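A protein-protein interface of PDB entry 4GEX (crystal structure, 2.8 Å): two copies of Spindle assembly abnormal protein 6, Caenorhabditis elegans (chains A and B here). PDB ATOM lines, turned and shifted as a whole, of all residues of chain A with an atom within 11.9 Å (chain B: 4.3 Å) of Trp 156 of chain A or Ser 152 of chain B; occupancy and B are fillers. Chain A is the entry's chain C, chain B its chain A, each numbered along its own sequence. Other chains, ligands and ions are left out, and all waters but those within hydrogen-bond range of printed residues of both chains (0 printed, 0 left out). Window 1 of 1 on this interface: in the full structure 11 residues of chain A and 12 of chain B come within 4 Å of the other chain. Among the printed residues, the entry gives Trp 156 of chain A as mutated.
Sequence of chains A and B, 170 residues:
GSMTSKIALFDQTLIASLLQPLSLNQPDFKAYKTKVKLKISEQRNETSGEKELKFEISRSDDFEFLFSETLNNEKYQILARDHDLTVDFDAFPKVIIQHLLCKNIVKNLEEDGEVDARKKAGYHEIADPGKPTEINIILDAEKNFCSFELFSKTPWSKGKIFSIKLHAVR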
ATOM      1  N   HIS A  83       6.706   2.201  12.798  1.00  0.00           N
ATOM      2  CA  HIS A  83       6.605   0.854  12.221  1.00  0.00           C
ATOM      3  C   HIS A  83       7.822   0.430  11.430  1.00  0.00           C
ATOM      4  O   HIS A  83       7.786  -0.626  10.789  1.00  0.00           O
ATOM      5  CB  HIS A  83       5.355   0.742  11.352  1.00  0.00           C
ATOM      6  CG  HIS A  83       4.120   1.037  12.129  1.00  0.00           C
ATOM      7  ND1 HIS A  83       3.520   2.279  12.068  1.00  0.00           N
ATOM      8  CD2 HIS A  83       3.480   0.299  13.063  1.00  0.00           C
ATOM      9  CE1 HIS A  83       2.493   2.233  12.898  1.00  0.00           C
ATOM     10  NE2 HIS A  83       2.443   1.079  13.544  1.00  0.00           N
ATOM     11  N   ASP A  84       8.909   1.202  11.518  1.00  0.00           N
ATOM     12  CA  ASP A  84      10.180   0.912  10.856  1.00  0.00           C
ATOM     13  C   ASP A  84      10.012   0.665   9.346  1.00  0.00           C
ATOM     14  O   ASP A  84      10.662  -0.209   8.767  1.00  0.00           O
ATOM     15  CB  ASP A  84      10.912  -0.268  11.539  1.00  0.00           C
ATOM     16  CG  ASP A  84      11.169  -0.049  13.015  1.00  0.00           C
ATOM     17  OD1 ASP A  84      12.000   0.836  13.348  1.00  0.00           O
ATOM     18  OD2 ASP A  84      10.468  -0.693  13.843  1.00  0.00           O
ATOM     19  N   LEU A  85       9.162   1.464   8.711  1.00  0.00           N
ATOM     20  CA  LEU A  85       8.959   1.380   7.263  1.00  0.00           C
ATOM     21  C   LEU A  85      10.164   1.990   6.563  1.00  0.00           C
ATOM     22  O   LEU A  85      10.659   3.031   7.015  1.00  0.00           O
ATOM     23  CB  LEU A  85       7.668   2.083   6.819  1.00  0.00           C
ATOM     24  CG  LEU A  85       6.384   1.691   7.534  1.00  0.00           C
ATOM     25  CD1 LEU A  85       5.188   2.542   7.046  1.00  0.00           C
ATOM     26  CD2 LEU A  85       6.136   0.194   7.406  1.00  0.00           C
ATOM     27  N   THR A  86      10.655   1.342   5.487  1.00  0.00           N
ATOM     28  CA  THR A  86      11.840   1.825   4.766  1.00  0.00           C
ATOM     29  C   THR A  86      11.447   2.415   3.417  1.00  0.00           C
ATOM     30  O   THR A  86      12.235   3.130   2.786  1.00  0.00           O
ATOM     31  CB  THR A  86      12.858   0.722   4.604  1.00  0.00           C
ATOM     32  OG1 THR A  86      12.264  -0.345   3.845  1.00  0.00           O
ATOM     33  CG2 THR A  86      13.404   0.238   5.940  1.00  0.00           C
ATOM     34  N   GLU A 134      -5.672 -10.778   8.320  1.00  0.00           N
ATOM     35  CA  GLU A 134      -4.510  -9.938   8.069  1.00  0.00           C
ATOM     36  C   GLU A 134      -4.852  -8.451   8.298  1.00  0.00           C
ATOM     37  O   GLU A 134      -3.950  -7.622   8.273  1.00  0.00           O
ATOM     38  CB  GLU A 134      -3.943 -10.197   6.658  1.00  0.00           C
ATOM     39  CG  GLU A 134      -3.457 -11.632   6.452  1.00  0.00           C
ATOM     40  CD  GLU A 134      -1.957 -11.876   6.387  1.00  0.00           C
ATOM     41  OE1 GLU A 134      -1.372 -11.607   5.311  1.00  0.00           O
ATOM     42  OE2 GLU A 134      -1.373 -12.367   7.387  1.00  0.00           O
ATOM     43  N   PHE A 151      -1.351  -6.641   8.562  1.00  0.00           N
ATOM     44  CA  PHE A 151      -0.333  -7.648   8.897  1.00  0.00           C
ATOM     45  C   PHE A 151       0.053  -8.543   7.748  1.00  0.00           C
ATOM     46  O   PHE A 151      -0.792  -8.878   6.931  1.00  0.00           O
ATOM     47  CB  PHE A 151      -0.870  -8.572   9.991  1.00  0.00           C
ATOM     48  CG  PHE A 151      -1.061  -7.939  11.334  1.00  0.00           C
ATOM     49  CD1 PHE A 151      -2.252  -7.316  11.659  1.00  0.00           C
ATOM     50  CD2 PHE A 151      -0.091  -8.055  12.312  1.00  0.00           C
ATOM     51  CE1 PHE A 151      -2.446  -6.767  12.920  1.00  0.00           C
ATOM     52  CE2 PHE A 151      -0.278  -7.493  13.570  1.00  0.00           C
ATOM     53  CZ  PHE A 151      -1.455  -6.854  13.866  1.00  0.00           C
ATOM     54  N   SER A 152       1.313  -8.992   7.720  1.00  0.00           N
ATOM     55  CA  SER A 152       1.806 -10.013   6.791  1.00  0.00           C
ATOM     56  C   SER A 152       2.545 -11.031   7.646  1.00  0.00           C
ATOM     57  O   SER A 152       3.715 -10.810   7.977  1.00  0.00           O
ATOM     58  CB  SER A 152       2.676  -9.422   5.688  1.00  0.00           C
ATOM     59  OG  SER A 152       2.929 -10.443   4.733  1.00  0.00           O
ATOM     60  N   LYS A 153       1.832 -12.091   8.101  1.00  0.00           N
ATOM     61  CA  LYS A 153       2.364 -13.112   9.021  1.00  0.00           C
ATOM     62  C   LYS A 153       3.680 -13.724   8.529  1.00  0.00           C
ATOM     63  O   LYS A 153       3.867 -13.918   7.322  1.00  0.00           O
ATOM     64  CB  LYS A 153       1.335 -14.227   9.246  1.00  0.00           C
ATOM     65  CG  LYS A 153       1.550 -14.983  10.542  1.00  0.00           C
ATOM     66  CD  LYS A 153       0.495 -16.032  10.820  1.00  0.00           C
ATOM     67  CE  LYS A 153       0.629 -16.525  12.246  1.00  0.00           C
ATOM     68  NZ  LYS A 153      -0.404 -17.539  12.602  1.00  0.00           N
ATOM     69  N   THR A 154       4.593 -13.983   9.468  1.00  0.00           N
ATOM     70  CA  THR A 154       5.878 -14.636   9.228  1.00  0.00           C
ATOM     71  C   THR A 154       5.939 -15.884  10.099  1.00  0.00           C
ATOM     72  O   THR A 154       5.210 -15.967  11.103  1.00  0.00           O
ATOM     73  CB  THR A 154       7.094 -13.732   9.566  1.00  0.00           C
ATOM     74  OG1 THR A 154       7.292 -13.704  10.985  1.00  0.00           O
ATOM     75  CG2 THR A 154       7.013 -12.373   8.999  1.00  0.00           C
ATOM     76  N   PRO A 155       6.921 -16.777   9.880  1.00  0.00           N
ATOM     77  CA  PRO A 155       7.020 -17.956  10.750  1.00  0.00           C
ATOM     78  C   PRO A 155       7.416 -17.634  12.190  1.00  0.00           C
ATOM     79  O   PRO A 155       7.339 -18.531  13.014  1.00  0.00           O
ATOM     80  CB  PRO A 155       8.111 -18.797  10.070  1.00  0.00           C
ATOM     81  CG  PRO A 155       8.124 -18.332   8.652  1.00  0.00           C
ATOM     82  CD  PRO A 155       7.889 -16.864   8.764  1.00  0.00           C
ATOM     83  N   TRP A 156       7.834 -16.389  12.504  1.00  0.00           N
ATOM     84  CA  TRP A 156       8.326 -16.060  13.868  1.00  0.00           C
ATOM     85  C   TRP A 156       7.601 -14.906  14.534  1.00  0.00           C
ATOM     86  O   TRP A 156       7.849 -14.668  15.709  1.00  0.00           O
ATOM     87  CB  TRP A 156       9.848 -15.718  13.846  1.00  0.00           C
ATOM     88  CG  TRP A 156      10.204 -14.758  12.743  1.00  0.00           C
ATOM     89  CD1 TRP A 156      10.063 -13.410  12.763  1.00  0.00           C
ATOM     90  CD2 TRP A 156      10.613 -15.101  11.409  1.00  0.00           C
ATOM     91  NE1 TRP A 156      10.353 -12.883  11.528  1.00  0.00           N
ATOM     92  CE2 TRP A 156      10.701 -13.896  10.676  1.00  0.00           C
ATOM     93  CE3 TRP A 156      10.974 -16.316  10.771  1.00  0.00           C
ATOM     94  CZ2 TRP A 156      11.104 -13.859   9.326  1.00  0.00           C
ATOM     95  CZ3 TRP A 156      11.367 -16.274   9.437  1.00  0.00           C
ATOM     96  CH2 TRP A 156      11.414 -15.055   8.726  1.00  0.00           C
ATOM     97  N   SER A 157       6.743 -14.175  13.816  1.00  0.00           N
ATOM     98  CA  SER A 157       6.062 -12.996  14.343  1.00  0.00           C
ATOM     99  C   SER A 157       4.744 -12.755  13.593  1.00  0.00           C
ATOM    100  O   SER A 157       4.540 -13.372  12.538  1.00  0.00           O
ATOM    101  CB  SER A 157       6.975 -11.786  14.178  1.00  0.00           C
ATOM    102  OG  SER A 157       7.102 -11.393  12.819  1.00  0.00           O
ATOM    103  N   LYS A 158       3.881 -11.827  14.100  1.00  0.00           N
ATOM    104  CA  LYS A 158       2.595 -11.467  13.488  1.00  0.00           C
ATOM    105  C   LYS A 158       2.789 -10.709  12.165  1.00  0.00           C
ATOM    106  O   LYS A 158       1.895 -10.711  11.306  1.00  0.00           O
ATOM    107  CB  LYS A 158       1.744 -10.634  14.447  1.00  0.00           C
ATOM    108  CG  LYS A 158       1.171 -11.414  15.637  1.00  0.00           C
ATOM    109  CD  LYS A 158       0.270 -10.590  16.574  1.00  0.00           C
ATOM    110  CE  LYS A 158      -1.152 -10.403  16.052  1.00  0.00           C
ATOM    111  NZ  LYS A 158      -1.890  -9.331  16.779  1.00  0.00           N
ATOM    112  N   GLY A 159       3.960 -10.084  12.016  1.00  0.00           N
ATOM    113  CA  GLY A 159       4.336  -9.339  10.823  1.00  0.00           C
ATOM    114  C   GLY A 159       3.557  -8.070  10.588  1.00  0.00           C
ATOM    115  O   GLY A 159       3.155  -7.803   9.459  1.00  0.00           O
ATOM    116  N   LYS A 160       3.328  -7.283  11.648  1.00  0.00           N
ATOM    117  CA  LYS A 160       2.602  -6.025  11.532  1.00  0.00           C
ATOM    118  C   LYS A 160       3.284  -5.141  10.495  1.00  0.00           C
ATOM    119  O   LYS A 160       4.501  -5.013  10.525  1.00  0.00           O
ATOM    120  CB  LYS A 160       2.530  -5.331  12.898  1.00  0.00           C
ATOM    121  CG  LYS A 160       1.613  -4.105  12.945  1.00  0.00           C
ATOM    122  CD  LYS A 160       1.038  -3.961  14.322  1.00  0.00           C
ATOM    123  CE  LYS A 160       0.747  -2.559  14.739  1.00  0.00           C
ATOM    124  NZ  LYS A 160       0.280  -2.535  16.160  1.00  0.00           N
ATOM    125  N   ILE A 161       2.522  -4.619   9.521  1.00  0.00           N
ATOM    126  CA  ILE A 161       3.074  -3.719   8.510  1.00  0.00           C
ATOM    127  C   ILE A 161       2.971  -2.315   9.066  1.00  0.00           C
ATOM    128  O   ILE A 161       4.001  -1.649   9.191  1.00  0.00           O
ATOM    129  CB  ILE A 161       2.438  -3.855   7.119  1.00  0.00           C
ATOM    130  CG1 ILE A 161       2.558  -5.301   6.617  1.00  0.00           C
ATOM    131  CG2 ILE A 161       3.085  -2.866   6.151  1.00  0.00           C
ATOM    132  CD1 ILE A 161       1.777  -5.615   5.348  1.00  0.00           C
ATOM    133  N   LEU B  85       8.549 -11.360  18.688  1.00  0.00           N
ATOM    134  CA  LEU B  85       8.525 -12.754  18.271  1.00  0.00           C
ATOM    135  C   LEU B  85       7.284 -13.412  18.859  1.00  0.00           C
ATOM    136  O   LEU B  85       6.966 -13.159  20.024  1.00  0.00           O
ATOM    137  CB  LEU B  85       9.797 -13.489  18.713  1.00  0.00           C
ATOM    138  CG  LEU B  85      11.134 -12.861  18.347  1.00  0.00           C
ATOM    139  CD1 LEU B  85      12.315 -13.711  18.867  1.00  0.00           C
ATOM    140  CD2 LEU B  85      11.229 -12.604  16.851  1.00  0.00           C
ATOM    141  N   THR B  86       6.578 -14.240  18.085  1.00  0.00           N
ATOM    142  CA  THR B  86       5.369 -14.896  18.598  1.00  0.00           C
ATOM    143  C   THR B  86       5.598 -16.392  18.780  1.00  0.00           C
ATOM    144  O   THR B  86       4.754 -17.090  19.368  1.00  0.00           O
ATOM    145  CB  THR B  86       4.159 -14.628  17.715  1.00  0.00           C
ATOM    146  OG1 THR B  86       4.435 -15.111  16.392  1.00  0.00           O
ATOM    147  CG2 THR B  86       3.760 -13.161  17.712  1.00  0.00           C
ATOM    148  N   VAL B  87       6.763 -16.885  18.333  1.00  0.00           N
ATOM    149  CA  VAL B  87       7.053 -18.298  18.513  1.00  0.00           C
ATOM    150  C   VAL B  87       7.635 -18.545  19.896  1.00  0.00           C
ATOM    151  O   VAL B  87       8.302 -17.673  20.468  1.00  0.00           O
ATOM    152  CB  VAL B  87       7.940 -18.897  17.425  1.00  0.00           C
ATOM    153  CG1 VAL B  87       7.262 -18.862  16.084  1.00  0.00           C
ATOM    154  CG2 VAL B  87       9.311 -18.260  17.394  1.00  0.00           C
ATOM    155  N   VAL B  95      12.540 -22.576  13.481  1.00  0.00           N
ATOM    156  CA  VAL B  95      12.079 -21.536  12.558  1.00  0.00           C
ATOM    157  C   VAL B  95      13.279 -20.733  11.984  1.00  0.00           C
ATOM    158  O   VAL B  95      13.365 -20.550  10.763  1.00  0.00           O
ATOM    159  CB  VAL B  95      11.051 -20.658  13.324  1.00  0.00           C
ATOM    160  CG1 VAL B  95      10.783 -19.332  12.649  1.00  0.00           C
ATOM    161  CG2 VAL B  95       9.766 -21.443  13.555  1.00  0.00           C
ATOM    162  N   HIS B  99      14.748 -20.862   8.186  1.00  0.00           N
ATOM    163  CA  HIS B  99      14.938 -19.630   7.441  1.00  0.00           C
ATOM    164  C   HIS B  99      16.331 -19.582   6.819  1.00  0.00           C
ATOM    165  O   HIS B  99      16.449 -19.334   5.624  1.00  0.00           O
ATOM    166  CB  HIS B  99      14.694 -18.402   8.326  1.00  0.00           C
ATOM    167  CG  HIS B  99      14.859 -17.112   7.581  1.00  0.00           C
ATOM    168  ND1 HIS B  99      15.914 -16.244   7.849  1.00  0.00           N
ATOM    169  CD2 HIS B  99      14.147 -16.621   6.537  1.00  0.00           C
ATOM    170  CE1 HIS B  99      15.796 -15.248   6.978  1.00  0.00           C
ATOM    171  NE2 HIS B  99      14.746 -15.433   6.170  1.00  0.00           N
ATOM    172  N   GLU B 134      21.884  -9.646   4.796  1.00  0.00           N
ATOM    173  CA  GLU B 134      20.841 -10.215   5.701  1.00  0.00           C
ATOM    174  C   GLU B 134      21.375 -10.528   7.133  1.00  0.00           C
ATOM    175  O   GLU B 134      20.561 -10.785   8.035  1.00  0.00           O
ATOM    176  CB  GLU B 134      20.092 -11.448   5.137  1.00  0.00           C
ATOM    177  CG  GLU B 134      19.410 -11.209   3.796  1.00  0.00           C
ATOM    178  CD  GLU B 134      17.892 -11.170   3.782  1.00  0.00           C
ATOM    179  OE1 GLU B 134      17.266 -12.252   3.883  1.00  0.00           O
ATOM    180  OE2 GLU B 134      17.335 -10.052   3.643  1.00  0.00           O
ATOM    181  N   PHE B 151      18.119 -10.530   9.438  1.00  0.00           N
ATOM    182  CA  PHE B 151      17.053  -9.854   8.692  1.00  0.00           C
ATOM    183  C   PHE B 151      16.438 -10.715   7.604  1.00  0.00           C
ATOM    184  O   PHE B 151      17.141 -11.494   6.953  1.00  0.00           O
ATOM    185  CB  PHE B 151      17.606  -8.610   7.995  1.00  0.00           C
ATOM    186  CG  PHE B 151      18.043  -7.493   8.886  1.00  0.00           C
ATOM    187  CD1 PHE B 151      19.342  -7.450   9.394  1.00  0.00           C
ATOM    188  CD2 PHE B 151      17.184  -6.447   9.178  1.00  0.00           C
ATOM    189  CE1 PHE B 151      19.758  -6.399  10.216  1.00  0.00           C
ATOM    190  CE2 PHE B 151      17.586  -5.403  10.015  1.00  0.00           C
ATOM    191  CZ  PHE B 151      18.870  -5.389  10.533  1.00  0.00           C
ATOM    192  N   SER B 152      15.137 -10.513   7.346  1.00  0.00           N
ATOM    193  CA  SER B 152      14.419 -11.096   6.210  1.00  0.00           C
ATOM    194  C   SER B 152      13.646  -9.963   5.539  1.00  0.00           C
ATOM    195  O   SER B 152      12.559  -9.591   6.013  1.00  0.00           O
ATOM    196  CB  SER B 152      13.508 -12.230   6.640  1.00  0.00           C
ATOM    197  OG  SER B 152      12.947 -12.854   5.498  1.00  0.00           O
ATOM    198  N   LYS B 153      14.239  -9.344   4.492  1.00  0.00           N
ATOM    199  CA  LYS B 153      13.666  -8.171   3.809  1.00  0.00           C
ATOM    200  C   LYS B 153      12.214  -8.369   3.351  1.00  0.00           C
ATOM    201  O   LYS B 153      11.852  -9.449   2.869  1.00  0.00           O
ATOM    202  CB  LYS B 153      14.510  -7.794   2.586  1.00  0.00           C
ATOM    203  CG  LYS B 153      14.403  -6.343   2.151  1.00  0.00           C
ATOM    204  CD  LYS B 153      15.172  -6.088   0.827  1.00  0.00           C
ATOM    205  CE  LYS B 153      14.452  -5.125  -0.122  1.00  0.00           C
ATOM    206  NZ  LYS B 153      13.270  -5.740  -0.818  1.00  0.00           N
ATOM    207  N   THR B 154      11.393  -7.308   3.500  1.00  0.00           N
ATOM    208  CA  THR B 154      10.019  -7.244   3.015  1.00  0.00           C
ATOM    209  C   THR B 154       9.950  -6.116   2.014  1.00  0.00           C
ATOM    210  O   THR B 154      10.848  -5.280   2.013  1.00  0.00           O
ATOM    211  CB  THR B 154       9.006  -7.022   4.147  1.00  0.00           C
ATOM    212  OG1 THR B 154       8.863  -5.631   4.366  1.00  0.00           O
ATOM    213  CG2 THR B 154       9.386  -7.685   5.420  1.00  0.00           C
ATOM    214  N   LYS B 158      13.113  -3.463   6.359  1.00  0.00           N
ATOM    215  CA  LYS B 158      14.343  -4.244   6.462  1.00  0.00           C
ATOM    216  C   LYS B 158      14.039  -5.680   6.935  1.00  0.00           C
ATOM    217  O   LYS B 158      14.785  -6.596   6.598  1.00  0.00           O
ATOM    218  CB  LYS B 158      15.329  -3.563   7.418  1.00  0.00           C
ATOM    219  CG  LYS B 158      16.058  -2.372   6.792  1.00  0.00           C
ATOM    220  CD  LYS B 158      16.933  -1.602   7.807  1.00  0.00           C
ATOM    221  CE  LYS B 158      18.315  -2.198   7.993  1.00  0.00           C
ATOM    222  NZ  LYS B 158      18.955  -1.795   9.285  1.00  0.00           N
ATOM    223  N   GLY B 159      12.961  -5.853   7.705  1.00  0.00           N
ATOM    224  CA  GLY B 159      12.518  -7.147   8.206  1.00  0.00           C
ATOM    225  C   GLY B 159      13.431  -7.764   9.229  1.00  0.00           C
ATOM    226  O   GLY B 159      13.780  -8.940   9.128  1.00  0.00           O
ATOM    227  N   ILE B 161      14.640  -9.721  12.168  1.00  0.00           N
ATOM    228  CA  ILE B 161      14.049 -10.842  12.886  1.00  0.00           C
ATOM    229  C   ILE B 161      14.376 -10.699  14.351  1.00  0.00           C
ATOM    230  O   ILE B 161      13.455 -10.682  15.168  1.00  0.00           O
ATOM    231  CB  ILE B 161      14.465 -12.207  12.334  1.00  0.00           C
ATOM    232  CG1 ILE B 161      14.138 -12.308  10.832  1.00  0.00           C
ATOM    233  CG2 ILE B 161      13.771 -13.305  13.139  1.00  0.00           C
ATOM    234  CD1 ILE B 161      14.654 -13.556  10.169  1.00  0.00           C
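The backbone carbonyl oxygen of Trp 156 of chain A sits at hydrogen-bond distance from the backbone NH of Thr 86 of chain B (2.7 Å).
O of Lys 158 of chain A lies close to N of Lys 153 of chain A (3.5 Å).
OG1 of Thr 154 of chain A lies close to N of Trp 156 of chain A (3.1 Å).
The side-chain hydroxyl (OG1) of Thr 154 of chain A sits at hydrogen-bond distance from the backbone NH (N) of Ser 157 of chain A, 2.9 Å away.
The backbone NH of Ser 152 of chain B is in hydrogen-bond range of the backbone carbonyl oxygen of Gly 159 of chain B, 2.7 Å away.
OG of Ser 152 of chain B is in hydrogen-bond range of NE2 of His 99 of chain B, at 3.2 Å.
OG of Ser 157 of chain A lies close to N of Gly 159 of chain A (3.5 Å).
CG2 of Thr 86 of chain A touches N of Lys 158 of chain B (3.7 Å).
O of Pro 155 of chain A touches CG1 of Val 87 of chain B, at 3.1 Å.
O of Pro 155 of chain A touches CG1 of Val 95 of chain B, at 3.6 Å.
Trp 156 of chain A touches Leu 85 of chain B.
N of Val 87 of chain B touches O of Trp 156 of chain A, 3.6 Å away.
CD2 of His 99 of chain B touches CH2 of Trp 156 of chain A, at 3.8 Å.
Ser 152 of chain B touches Trp 156 of chain A.
Ile 161 of chain B touches Trp 156 of chain A.
Ser 157 of chain A touches Thr 86 of chain B (CA to OG1, 3.4 Å).
Thr 86 of chain B touches Lys 158 of chain A.
Trp 156 of chain A touches just these residues of chain B: Leu 85 (3.3 Å), Thr 86 (2.7 Å), Val 87 (3.6 Å), Val 95 (3.6 Å), His 99 (3.8 Å), Ser 152 (3.96 Å) and Ile 161 (3.7 Å).
Ser 152 of chain B touches just one residue of chain A: Trp 156.
Of chain A, only Trp 156 comes within 4 Å of Leu 85 of chain B.
Val 87 of chain B touches just these residues of chain A: Pro 155 and Trp 156.
His 99 of chain B touches one residue of chain A.
No residue of chain A comes within 4 Å of Phe 151 of chain B.
No residue of chain A comes within 4 Å of Lys 153 of chain B.
Of chain A, only Trp 156 (3.7 Å) comes within 4 Å of Ile 161 of chain B.
Printed residues of chain B within 4 Å of Ser 157 of chain A: Thr 86.
Printed residues of chain B within 4 Å of Lys 158 of chain A: Thr 86.
Of the printed residues of chain A, Lys 158 of chain B touches Thr 86 (3.7 Å).
The nearest residue of chain A that does not touch Ser 152 of chain B is Thr 154 of chain A (6.9 Å).
The nearest printed residue of chain B that does not touch Lys 158 of chain A is Leu 85 of chain B (6.1 Å).
Hydrophobic or aromatic side chains of chain A within 4 Å of the printed part of chain B: Pro 155 and Trp 156.
Of the 13 printed residues of chain B, 8 touch a printed residue of chain A.
Along chain B the printed residues that touch a printed residue of chain A span positions 85 to 161.
Among the printed residues, 12 pairs touch across the chains.
Among the printed residues, no Asp or Glu carboxylate lies within 4 Å of a Lys or Arg side-chain nitrogen of the other chain.
Thr 86 of chain A touches Lys 158 of chain B, and with the chains exchanged Lys 158 of chain A touches Thr 86 of chain B.
Positions printed for both chains: 85, 86, 134, 151, 152, 153, 154, 158, 159 and 161.
Of the 12 pairs that touch across the chains among the printed residues, 2 have their exchanged pair printed and touching as well.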
